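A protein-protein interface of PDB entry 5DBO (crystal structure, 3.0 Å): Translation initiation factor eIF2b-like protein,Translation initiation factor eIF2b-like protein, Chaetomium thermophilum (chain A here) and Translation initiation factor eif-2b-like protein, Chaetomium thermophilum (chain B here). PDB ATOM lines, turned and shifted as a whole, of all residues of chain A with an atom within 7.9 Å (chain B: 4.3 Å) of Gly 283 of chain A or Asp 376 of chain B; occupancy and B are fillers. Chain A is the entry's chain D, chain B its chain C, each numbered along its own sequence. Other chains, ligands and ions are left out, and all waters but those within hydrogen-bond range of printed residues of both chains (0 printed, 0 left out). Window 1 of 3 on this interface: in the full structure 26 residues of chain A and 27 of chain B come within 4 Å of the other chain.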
ATOM      1  N   TYR A 224     -11.678  27.630  37.835  1.00  0.00           N
ATOM      2  CA  TYR A 224     -11.689  28.712  36.844  1.00  0.00           C
ATOM      3  C   TYR A 224     -10.899  29.932  37.325  1.00  0.00           C
ATOM      4  O   TYR A 224     -11.189  30.485  38.389  1.00  0.00           O
ATOM      5  CB  TYR A 224     -13.111  29.132  36.487  1.00  0.00           C
ATOM      6  CG  TYR A 224     -13.168  30.020  35.261  1.00  0.00           C
ATOM      7  CD1 TYR A 224     -13.281  29.468  33.991  1.00  0.00           C
ATOM      8  CD2 TYR A 224     -13.093  31.399  35.366  1.00  0.00           C
ATOM      9  CE1 TYR A 224     -13.326  30.261  32.864  1.00  0.00           C
ATOM     10  CE2 TYR A 224     -13.137  32.201  34.243  1.00  0.00           C
ATOM     11  CZ  TYR A 224     -13.253  31.625  32.998  1.00  0.00           C
ATOM     12  OH  TYR A 224     -13.303  32.413  31.875  1.00  0.00           O
ATOM     13  N   ALA A 248      -9.407  26.302  33.608  1.00  0.00           N
ATOM     14  CA  ALA A 248     -10.030  27.111  32.572  1.00  0.00           C
ATOM     15  C   ALA A 248      -9.718  28.592  32.769  1.00  0.00           C
ATOM     16  O   ALA A 248      -9.772  29.096  33.886  1.00  0.00           O
ATOM     17  CB  ALA A 248     -11.527  26.881  32.558  1.00  0.00           C
ATOM     18  N   SER A 249      -9.361  29.269  31.681  1.00  0.00           N
ATOM     19  CA  SER A 249      -9.107  30.708  31.695  1.00  0.00           C
ATOM     20  C   SER A 249      -9.912  31.395  30.588  1.00  0.00           C
ATOM     21  O   SER A 249     -10.208  30.784  29.559  1.00  0.00           O
ATOM     22  CB  SER A 249      -7.614  31.003  31.537  1.00  0.00           C
ATOM     23  OG  SER A 249      -7.044  30.236  30.490  1.00  0.00           O
ATOM     24  N   LEU A 250     -10.277  32.655  30.806  1.00  0.00           N
ATOM     25  CA  LEU A 250     -11.126  33.380  29.863  1.00  0.00           C
ATOM     26  C   LEU A 250     -10.454  33.624  28.523  1.00  0.00           C
ATOM     27  O   LEU A 250     -11.033  33.375  27.467  1.00  0.00           O
ATOM     28  CB  LEU A 250     -11.536  34.736  30.444  1.00  0.00           C
ATOM     29  CG  LEU A 250     -12.437  35.585  29.538  1.00  0.00           C
ATOM     30  CD1 LEU A 250     -13.690  34.825  29.128  1.00  0.00           C
ATOM     31  CD2 LEU A 250     -12.793  36.905  30.183  1.00  0.00           C
ATOM     32  N   LEU A 279      -7.398  23.941  29.823  1.00  0.00           N
ATOM     33  CA  LEU A 279      -8.315  24.137  28.714  1.00  0.00           C
ATOM     34  C   LEU A 279      -8.057  25.449  27.992  1.00  0.00           C
ATOM     35  O   LEU A 279      -8.114  26.526  28.591  1.00  0.00           O
ATOM     36  CB  LEU A 279      -9.754  24.105  29.219  1.00  0.00           C
ATOM     37  CG  LEU A 279     -10.339  22.707  29.382  1.00  0.00           C
ATOM     38  CD1 LEU A 279     -11.803  22.790  29.755  1.00  0.00           C
ATOM     39  CD2 LEU A 279     -10.150  21.914  28.101  1.00  0.00           C
ATOM     40  N   ALA A 280      -7.781  25.353  26.697  1.00  0.00           N
ATOM     41  CA  ALA A 280      -7.632  26.532  25.861  1.00  0.00           C
ATOM     42  C   ALA A 280      -8.945  26.846  25.159  1.00  0.00           C
ATOM     43  O   ALA A 280      -8.960  27.341  24.033  1.00  0.00           O
ATOM     44  CB  ALA A 280      -6.523  26.332  24.852  1.00  0.00           C
ATOM     45  N   SER A 281     -10.051  26.528  25.820  1.00  0.00           N
ATOM     46  CA  SER A 281     -11.365  26.833  25.276  1.00  0.00           C
ATOM     47  C   SER A 281     -12.038  27.962  26.047  1.00  0.00           C
ATOM     48  O   SER A 281     -12.004  28.002  27.274  1.00  0.00           O
ATOM     49  CB  SER A 281     -12.251  25.585  25.285  1.00  0.00           C
ATOM     50  OG  SER A 281     -13.606  25.913  25.034  1.00  0.00           O
ATOM     51  N   ASN A 282     -12.638  28.885  25.308  1.00  0.00           N
ATOM     52  CA  ASN A 282     -13.566  29.846  25.878  1.00  0.00           C
ATOM     53  C   ASN A 282     -14.983  29.342  25.643  1.00  0.00           C
ATOM     54  O   ASN A 282     -15.398  29.144  24.500  1.00  0.00           O
ATOM     55  CB  ASN A 282     -13.366  31.227  25.263  1.00  0.00           C
ATOM     56  CG  ASN A 282     -14.487  32.181  25.608  1.00  0.00           C
ATOM     57  OD1 ASN A 282     -15.378  32.424  24.789  1.00  0.00           O
ATOM     58  ND2 ASN A 282     -14.463  32.716  26.828  1.00  0.00           N
ATOM     59  N   GLY A 283     -15.729  29.150  26.723  1.00  0.00           N
ATOM     60  CA  GLY A 283     -16.993  28.441  26.654  1.00  0.00           C
ATOM     61  C   GLY A 283     -16.748  27.020  27.134  1.00  0.00           C
ATOM     62  O   GLY A 283     -15.968  26.272  26.535  1.00  0.00           O
ATOM     63  N   LEU A 284     -17.403  26.655  28.234  1.00  0.00           N
ATOM     64  CA  LEU A 284     -17.076  25.429  28.954  1.00  0.00           C
ATOM     65  C   LEU A 284     -18.189  24.395  28.920  1.00  0.00           C
ATOM     66  O   LEU A 284     -18.101  23.352  29.568  1.00  0.00           O
ATOM     67  CB  LEU A 284     -16.725  25.755  30.409  1.00  0.00           C
ATOM     68  CG  LEU A 284     -15.365  26.380  30.742  1.00  0.00           C
ATOM     69  CD1 LEU A 284     -15.105  27.710  30.040  1.00  0.00           C
ATOM     70  CD2 LEU A 284     -15.267  26.555  32.246  1.00  0.00           C
ATOM     71  N   MET A 285     -19.223  24.680  28.142  1.00  0.00           N
ATOM     72  CA  MET A 285     -20.400  23.822  28.062  1.00  0.00           C
ATOM     73  C   MET A 285     -20.068  22.387  27.605  1.00  0.00           C
ATOM     74  O   MET A 285     -20.741  21.434  28.001  1.00  0.00           O
ATOM     75  CB  MET A 285     -21.428  24.448  27.122  1.00  0.00           C
ATOM     76  CG  MET A 285     -22.814  23.872  27.270  1.00  0.00           C
ATOM     77  SD  MET A 285     -23.531  24.325  28.862  1.00  0.00           S
ATOM     78  CE  MET A 285     -25.164  23.589  28.731  1.00  0.00           C
ATOM     79  N   ALA A 286     -19.059  22.244  26.747  1.00  0.00           N
ATOM     80  CA  ALA A 286     -18.643  20.930  26.243  1.00  0.00           C
ATOM     81  C   ALA A 286     -18.035  20.013  27.317  1.00  0.00           C
ATOM     82  O   ALA A 286     -18.215  18.794  27.275  1.00  0.00           O
ATOM     83  CB  ALA A 286     -17.654  21.100  25.088  1.00  0.00           C
ATOM     84  N   TYR A 287     -17.295  20.589  28.258  1.00  0.00           N
ATOM     85  CA  TYR A 287     -16.539  19.788  29.222  1.00  0.00           C
ATOM     86  C   TYR A 287     -17.224  19.608  30.577  1.00  0.00           C
ATOM     87  O   TYR A 287     -16.829  18.742  31.360  1.00  0.00           O
ATOM     88  CB  TYR A 287     -15.153  20.397  29.437  1.00  0.00           C
ATOM     89  CG  TYR A 287     -14.489  20.895  28.173  1.00  0.00           C
ATOM     90  CD1 TYR A 287     -13.715  20.045  27.391  1.00  0.00           C
ATOM     91  CD2 TYR A 287     -14.627  22.215  27.765  1.00  0.00           C
ATOM     92  CE1 TYR A 287     -13.101  20.497  26.239  1.00  0.00           C
ATOM     93  CE2 TYR A 287     -14.017  22.677  26.618  1.00  0.00           C
ATOM     94  CZ  TYR A 287     -13.254  21.816  25.856  1.00  0.00           C
ATOM     95  OH  TYR A 287     -12.646  22.279  24.704  1.00  0.00           O
ATOM     96  N   ILE A 288     -18.238  20.420  30.858  1.00  0.00           N
ATOM     97  CA  ILE A 288     -18.890  20.409  32.171  1.00  0.00           C
ATOM     98  C   ILE A 288     -19.420  19.047  32.665  1.00  0.00           C
ATOM     99  O   ILE A 288     -19.212  18.704  33.832  1.00  0.00           O
ATOM    100  CB  ILE A 288     -20.059  21.417  32.195  1.00  0.00           C
ATOM    101  CG1 ILE A 288     -19.514  22.824  32.371  1.00  0.00           C
ATOM    102  CG2 ILE A 288     -21.012  21.124  33.334  1.00  0.00           C
ATOM    103  CD1 ILE A 288     -18.850  23.025  33.720  1.00  0.00           C
ATOM    104  N   GLY A 312     -15.866  35.882  32.850  1.00  0.00           N
ATOM    105  CA  GLY A 312     -15.940  34.566  32.250  1.00  0.00           C
ATOM    106  C   GLY A 312     -16.153  33.463  33.264  1.00  0.00           C
ATOM    107  O   GLY A 312     -16.398  32.317  32.894  1.00  0.00           O
ATOM    108  N   CYS A 314     -18.662  33.402  35.167  1.00  0.00           N
ATOM    109  CA  CYS A 314     -20.099  33.199  35.183  1.00  0.00           C
ATOM    110  C   CYS A 314     -20.533  32.150  34.154  1.00  0.00           C
ATOM    111  O   CYS A 314     -21.496  31.429  34.380  1.00  0.00           O
ATOM    112  CB  CYS A 314     -20.821  34.525  34.931  1.00  0.00           C
ATOM    113  SG  CYS A 314     -22.576  34.512  35.354  1.00  0.00           S
ATOM    114  N   ILE A 315     -19.821  32.041  33.038  1.00  0.00           N
ATOM    115  CA  ILE A 315     -20.190  31.036  32.047  1.00  0.00           C
ATOM    116  C   ILE A 315     -19.927  29.646  32.626  1.00  0.00           C
ATOM    117  O   ILE A 315     -20.699  28.705  32.402  1.00  0.00           O
ATOM    118  CB  ILE A 315     -19.447  31.234  30.693  1.00  0.00           C
ATOM    119  CG1 ILE A 315     -18.014  30.707  30.742  1.00  0.00           C
ATOM    120  CG2 ILE A 315     -19.471  32.700  30.279  1.00  0.00           C
ATOM    121  CD1 ILE A 315     -17.218  31.010  29.502  1.00  0.00           C
ATOM    122  N   ALA A 316     -18.856  29.537  33.402  1.00  0.00           N
ATOM    123  CA  ALA A 316     -18.529  28.294  34.075  1.00  0.00           C
ATOM    124  C   ALA A 316     -19.593  27.984  35.114  1.00  0.00           C
ATOM    125  O   ALA A 316     -20.068  26.853  35.199  1.00  0.00           O
ATOM    126  CB  ALA A 316     -17.159  28.382  34.724  1.00  0.00           C
ATOM    127  N   GLN A 318     -22.763  29.052  35.332  1.00  0.00           N
ATOM    128  CA  GLN A 318     -24.067  28.775  34.751  1.00  0.00           C
ATOM    129  C   GLN A 318     -24.081  27.388  34.113  1.00  0.00           C
ATOM    130  O   GLN A 318     -25.016  26.588  34.321  1.00  0.00           O
ATOM    131  CB  GLN A 318     -24.419  29.860  33.736  1.00  0.00           C
ATOM    132  CG  GLN A 318     -25.892  30.004  33.455  1.00  0.00           C
ATOM    133  CD  GLN A 318     -26.212  31.341  32.824  1.00  0.00           C
ATOM    134  OE1 GLN A 318     -25.310  32.103  32.471  1.00  0.00           O
ATOM    135  NE2 GLN A 318     -27.501  31.630  32.664  1.00  0.00           N
ATOM    136  N   ALA A 319     -23.031  27.103  33.344  1.00  0.00           N
ATOM    137  CA  ALA A 319     -22.891  25.796  32.715  1.00  0.00           C
ATOM    138  C   ALA A 319     -22.911  24.700  33.773  1.00  0.00           C
ATOM    139  O   ALA A 319     -23.558  23.669  33.600  1.00  0.00           O
ATOM    140  CB  ALA A 319     -21.616  25.731  31.910  1.00  0.00           C
ATOM    141  N   ALA A 320     -22.207  24.945  34.877  1.00  0.00           N
ATOM    142  CA  ALA A 320     -22.182  24.020  36.007  1.00  0.00           C
ATOM    143  C   ALA A 320     -23.556  23.883  36.645  1.00  0.00           C
ATOM    144  O   ALA A 320     -23.979  22.786  37.016  1.00  0.00           O
ATOM    145  CB  ALA A 320     -21.180  24.481  37.045  1.00  0.00           C
ATOM    146  N   LEU B 342     -16.638  35.487  25.710  1.00  0.00           N
ATOM    147  CA  LEU B 342     -17.966  35.186  26.228  1.00  0.00           C
ATOM    148  C   LEU B 342     -18.149  35.693  27.651  1.00  0.00           C
ATOM    149  O   LEU B 342     -19.104  35.315  28.327  1.00  0.00           O
ATOM    150  CB  LEU B 342     -18.202  33.678  26.197  1.00  0.00           C
ATOM    151  CG  LEU B 342     -18.604  33.068  24.857  1.00  0.00           C
ATOM    152  CD1 LEU B 342     -18.894  31.583  25.042  1.00  0.00           C
ATOM    153  CD2 LEU B 342     -19.792  33.797  24.263  1.00  0.00           C
ATOM    154  N   LEU B 345     -21.573  37.511  29.623  1.00  0.00           N
ATOM    155  CA  LEU B 345     -22.555  37.023  28.664  1.00  0.00           C
ATOM    156  C   LEU B 345     -23.993  37.405  29.002  1.00  0.00           C
ATOM    157  O   LEU B 345     -24.756  37.797  28.123  1.00  0.00           O
ATOM    158  CB  LEU B 345     -22.450  35.502  28.563  1.00  0.00           C
ATOM    159  CG  LEU B 345     -23.178  34.860  27.395  1.00  0.00           C
ATOM    160  CD1 LEU B 345     -22.814  35.610  26.151  1.00  0.00           C
ATOM    161  CD2 LEU B 345     -22.775  33.409  27.272  1.00  0.00           C
ATOM    162  N   GLY B 373     -18.191  27.076  22.004  1.00  0.00           N
ATOM    163  CA  GLY B 373     -18.708  28.281  22.625  1.00  0.00           C
ATOM    164  C   GLY B 373     -20.169  28.509  22.285  1.00  0.00           C
ATOM    165  O   GLY B 373     -20.866  29.259  22.967  1.00  0.00           O
ATOM    166  N   THR B 374     -20.637  27.833  21.239  1.00  0.00           N
ATOM    167  CA  THR B 374     -22.011  27.981  20.765  1.00  0.00           C
ATOM    168  C   THR B 374     -23.043  27.615  21.824  1.00  0.00           C
ATOM    169  O   THR B 374     -23.971  28.388  22.098  1.00  0.00           O
ATOM    170  CB  THR B 374     -22.270  27.105  19.518  1.00  0.00           C
ATOM    171  OG1 THR B 374     -21.712  27.731  18.354  1.00  0.00           O
ATOM    172  CG2 THR B 374     -23.756  26.914  19.299  1.00  0.00           C
ATOM    173  N   ALA B 375     -22.872  26.443  22.427  1.00  0.00           N
ATOM    174  CA  ALA B 375     -23.838  25.943  23.392  1.00  0.00           C
ATOM    175  C   ALA B 375     -23.960  26.874  24.587  1.00  0.00           C
ATOM    176  O   ALA B 375     -25.034  26.996  25.173  1.00  0.00           O
ATOM    177  CB  ALA B 375     -23.462  24.546  23.847  1.00  0.00           C
ATOM    178  N   ASP B 376     -22.861  27.533  24.942  1.00  0.00           N
ATOM    179  CA  ASP B 376     -22.878  28.478  26.053  1.00  0.00           C
ATOM    180  C   ASP B 376     -23.797  29.653  25.731  1.00  0.00           C
ATOM    181  O   ASP B 376     -24.624  30.048  26.553  1.00  0.00           O
ATOM    182  CB  ASP B 376     -21.465  28.965  26.377  1.00  0.00           C
ATOM    183  CG  ASP B 376     -20.540  27.833  26.796  1.00  0.00           C
ATOM    184  OD1 ASP B 376     -20.360  27.622  28.016  1.00  0.00           O
ATOM    185  OD2 ASP B 376     -20.011  27.137  25.904  1.00  0.00           O
ATOM    186  N   VAL B 377     -23.651  30.207  24.532  1.00  0.00           N
ATOM    187  CA  VAL B 377     -24.497  31.316  24.105  1.00  0.00           C
ATOM    188  C   VAL B 377     -25.958  30.881  24.038  1.00  0.00           C
ATOM    189  O   VAL B 377     -26.851  31.596  24.501  1.00  0.00           O
ATOM    190  CB  VAL B 377     -24.070  31.858  22.731  1.00  0.00           C
ATOM    191  CG1 VAL B 377     -24.939  33.036  22.334  1.00  0.00           C
ATOM    192  CG2 VAL B 377     -22.604  32.255  22.755  1.00  0.00           C
ATOM    193  N   ALA B 378     -26.188  29.693  23.485  1.00  0.00           N
ATOM    194  CA  ALA B 378     -27.543  29.166  23.341  1.00  0.00           C
ATOM    195  C   ALA B 378     -28.231  28.971  24.696  1.00  0.00           C
ATOM    196  O   ALA B 378     -29.391  29.339  24.865  1.00  0.00           O
ATOM    197  CB  ALA B 378     -27.519  27.861  22.568  1.00  0.00           C
ATOM    198  N   MET B 379     -27.516  28.395  25.657  1.00  0.00           N
ATOM    199  CA  MET B 379     -28.066  28.197  26.998  1.00  0.00           C
ATOM    200  C   MET B 379     -28.308  29.535  27.694  1.00  0.00           C
ATOM    201  O   MET B 379     -29.360  29.750  28.291  1.00  0.00           O
ATOM    202  CB  MET B 379     -27.133  27.330  27.857  1.00  0.00           C
ATOM    203  CG  MET B 379     -27.351  27.491  29.367  1.00  0.00           C
ATOM    204  SD  MET B 379     -25.878  27.191  30.347  1.00  0.00           S
ATOM    205  CE  MET B 379     -24.763  28.428  29.683  1.00  0.00           C
ATOM    206  N   ALA B 380     -27.320  30.420  27.632  1.00  0.00           N
ATOM    207  CA  ALA B 380     -27.438  31.724  28.261  1.00  0.00           C
ATOM    208  C   ALA B 380     -28.684  32.433  27.744  1.00  0.00           C
ATOM    209  O   ALA B 380     -29.478  32.983  28.521  1.00  0.00           O
ATOM    210  CB  ALA B 380     -26.194  32.558  27.998  1.00  0.00           C
ATOM    211  N   ASP B 427     -18.729  22.042  19.756  1.00  0.00           N
ATOM    212  CA  ASP B 427     -19.548  21.610  20.881  1.00  0.00           C
ATOM    213  C   ASP B 427     -20.977  21.282  20.444  1.00  0.00           C
ATOM    214  O   ASP B 427     -21.417  21.644  19.336  1.00  0.00           O
ATOM    215  CB  ASP B 427     -19.556  22.674  21.983  1.00  0.00           C
ATOM    216  CG  ASP B 427     -20.228  23.960  21.554  1.00  0.00           C
ATOM    217  OD1 ASP B 427     -20.374  24.184  20.334  1.00  0.00           O
ATOM    218  OD2 ASP B 427     -20.595  24.761  22.438  1.00  0.00           O
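Of the printed residues of chain B, Gly 283 of chain A touches Asp 376 (3.4 Å). Asp 376 of chain B touches three residues of chain A. Printed residues of chain B within 4 Å of Met 285 of chain A: Ala 375, Asp 376 and Met 379. Printed residues of chain A within 4 Å of Asp 427 of chain B: Ala 286. Printed residues of chain A within 4 Å of Gly 373 of chain B: Asn 282. Of the printed residues of chain B, Ile 315 of chain A touches Leu 342. Ala 380 of chain B touches none of the printed residues of chain A.
The backbone carbonyl oxygen of Gly 283 of chain A lies within hydrogen-bond range of the side-chain hydroxyl of Ser 281 of chain A (2.8 Å). The side-chain carboxylate (OD2) of Asp 427 of chain B is in hydrogen-bond range of the backbone NH (N) of Gly 373 of chain B, 3.4 Å away. The backbone NH of Thr 374 of chain B is in hydrogen-bond range of the side-chain carboxylate of Asp 427 of chain B, at 3.3 Å. The backbone NH (N) of Ala 375 of chain B lies within hydrogen-bond range of the side-chain carboxylate (OD2) of Asp 427 of chain B, at 2.8 Å.
Of the 21 printed residues of chain A, 6 touch a printed residue of chain B. Printed residues of chain A that touch a printed residue of chain B: Asn 282, Gly 283, Leu 284, Met 285, Ala 286 and Ile 315. Hydrophobic or aromatic side chains of chain A within 4 Å of the printed part of chain B: Met 285, Ala 286 and Ile 315. Printed residues of chain B that touch a printed residue of chain A: Leu 342, Gly 373, Ala 375, Asp 376, Met 379 and Asp 427. Among the printed residues, 9 pairs touch across the chains. Among the printed residues, no Asp or Glu carboxylate lies within 4 Å of a Lys or Arg side-chain nitrogen of the other chain.
The backbone NH (N) of Leu 342 of chain B lies close to the side-chain amide oxygen (OD1) of Asn 282 of chain A. The side-chain carboxylate of Asp 376 of chain B is in hydrogen-bond range of the backbone NH of Met 285 of chain A (3.2 Å). The side-chain carboxylate of Asp 376 of chain B sits at hydrogen-bond distance from the backbone NH of Leu 284 of chain A, 3.1 Å away.
Among the printed residues, merely in contact across the chains: Asn 282 of chain A with Gly 373 of chain B (3.9 Å), Gly 283 of chain A with Asp 376 of chain B (3.4 Å), Met 285 of chain A with Ala 375 of chain B (3.5 Å), Met 285 of chain A with Met 379 of chain B (3.99 Å), Ala 286 of chain A with Asp 427 of chain B (3.97 Å) and Ile 315 of chain A with Leu 342 of chain B (3.3 Å).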
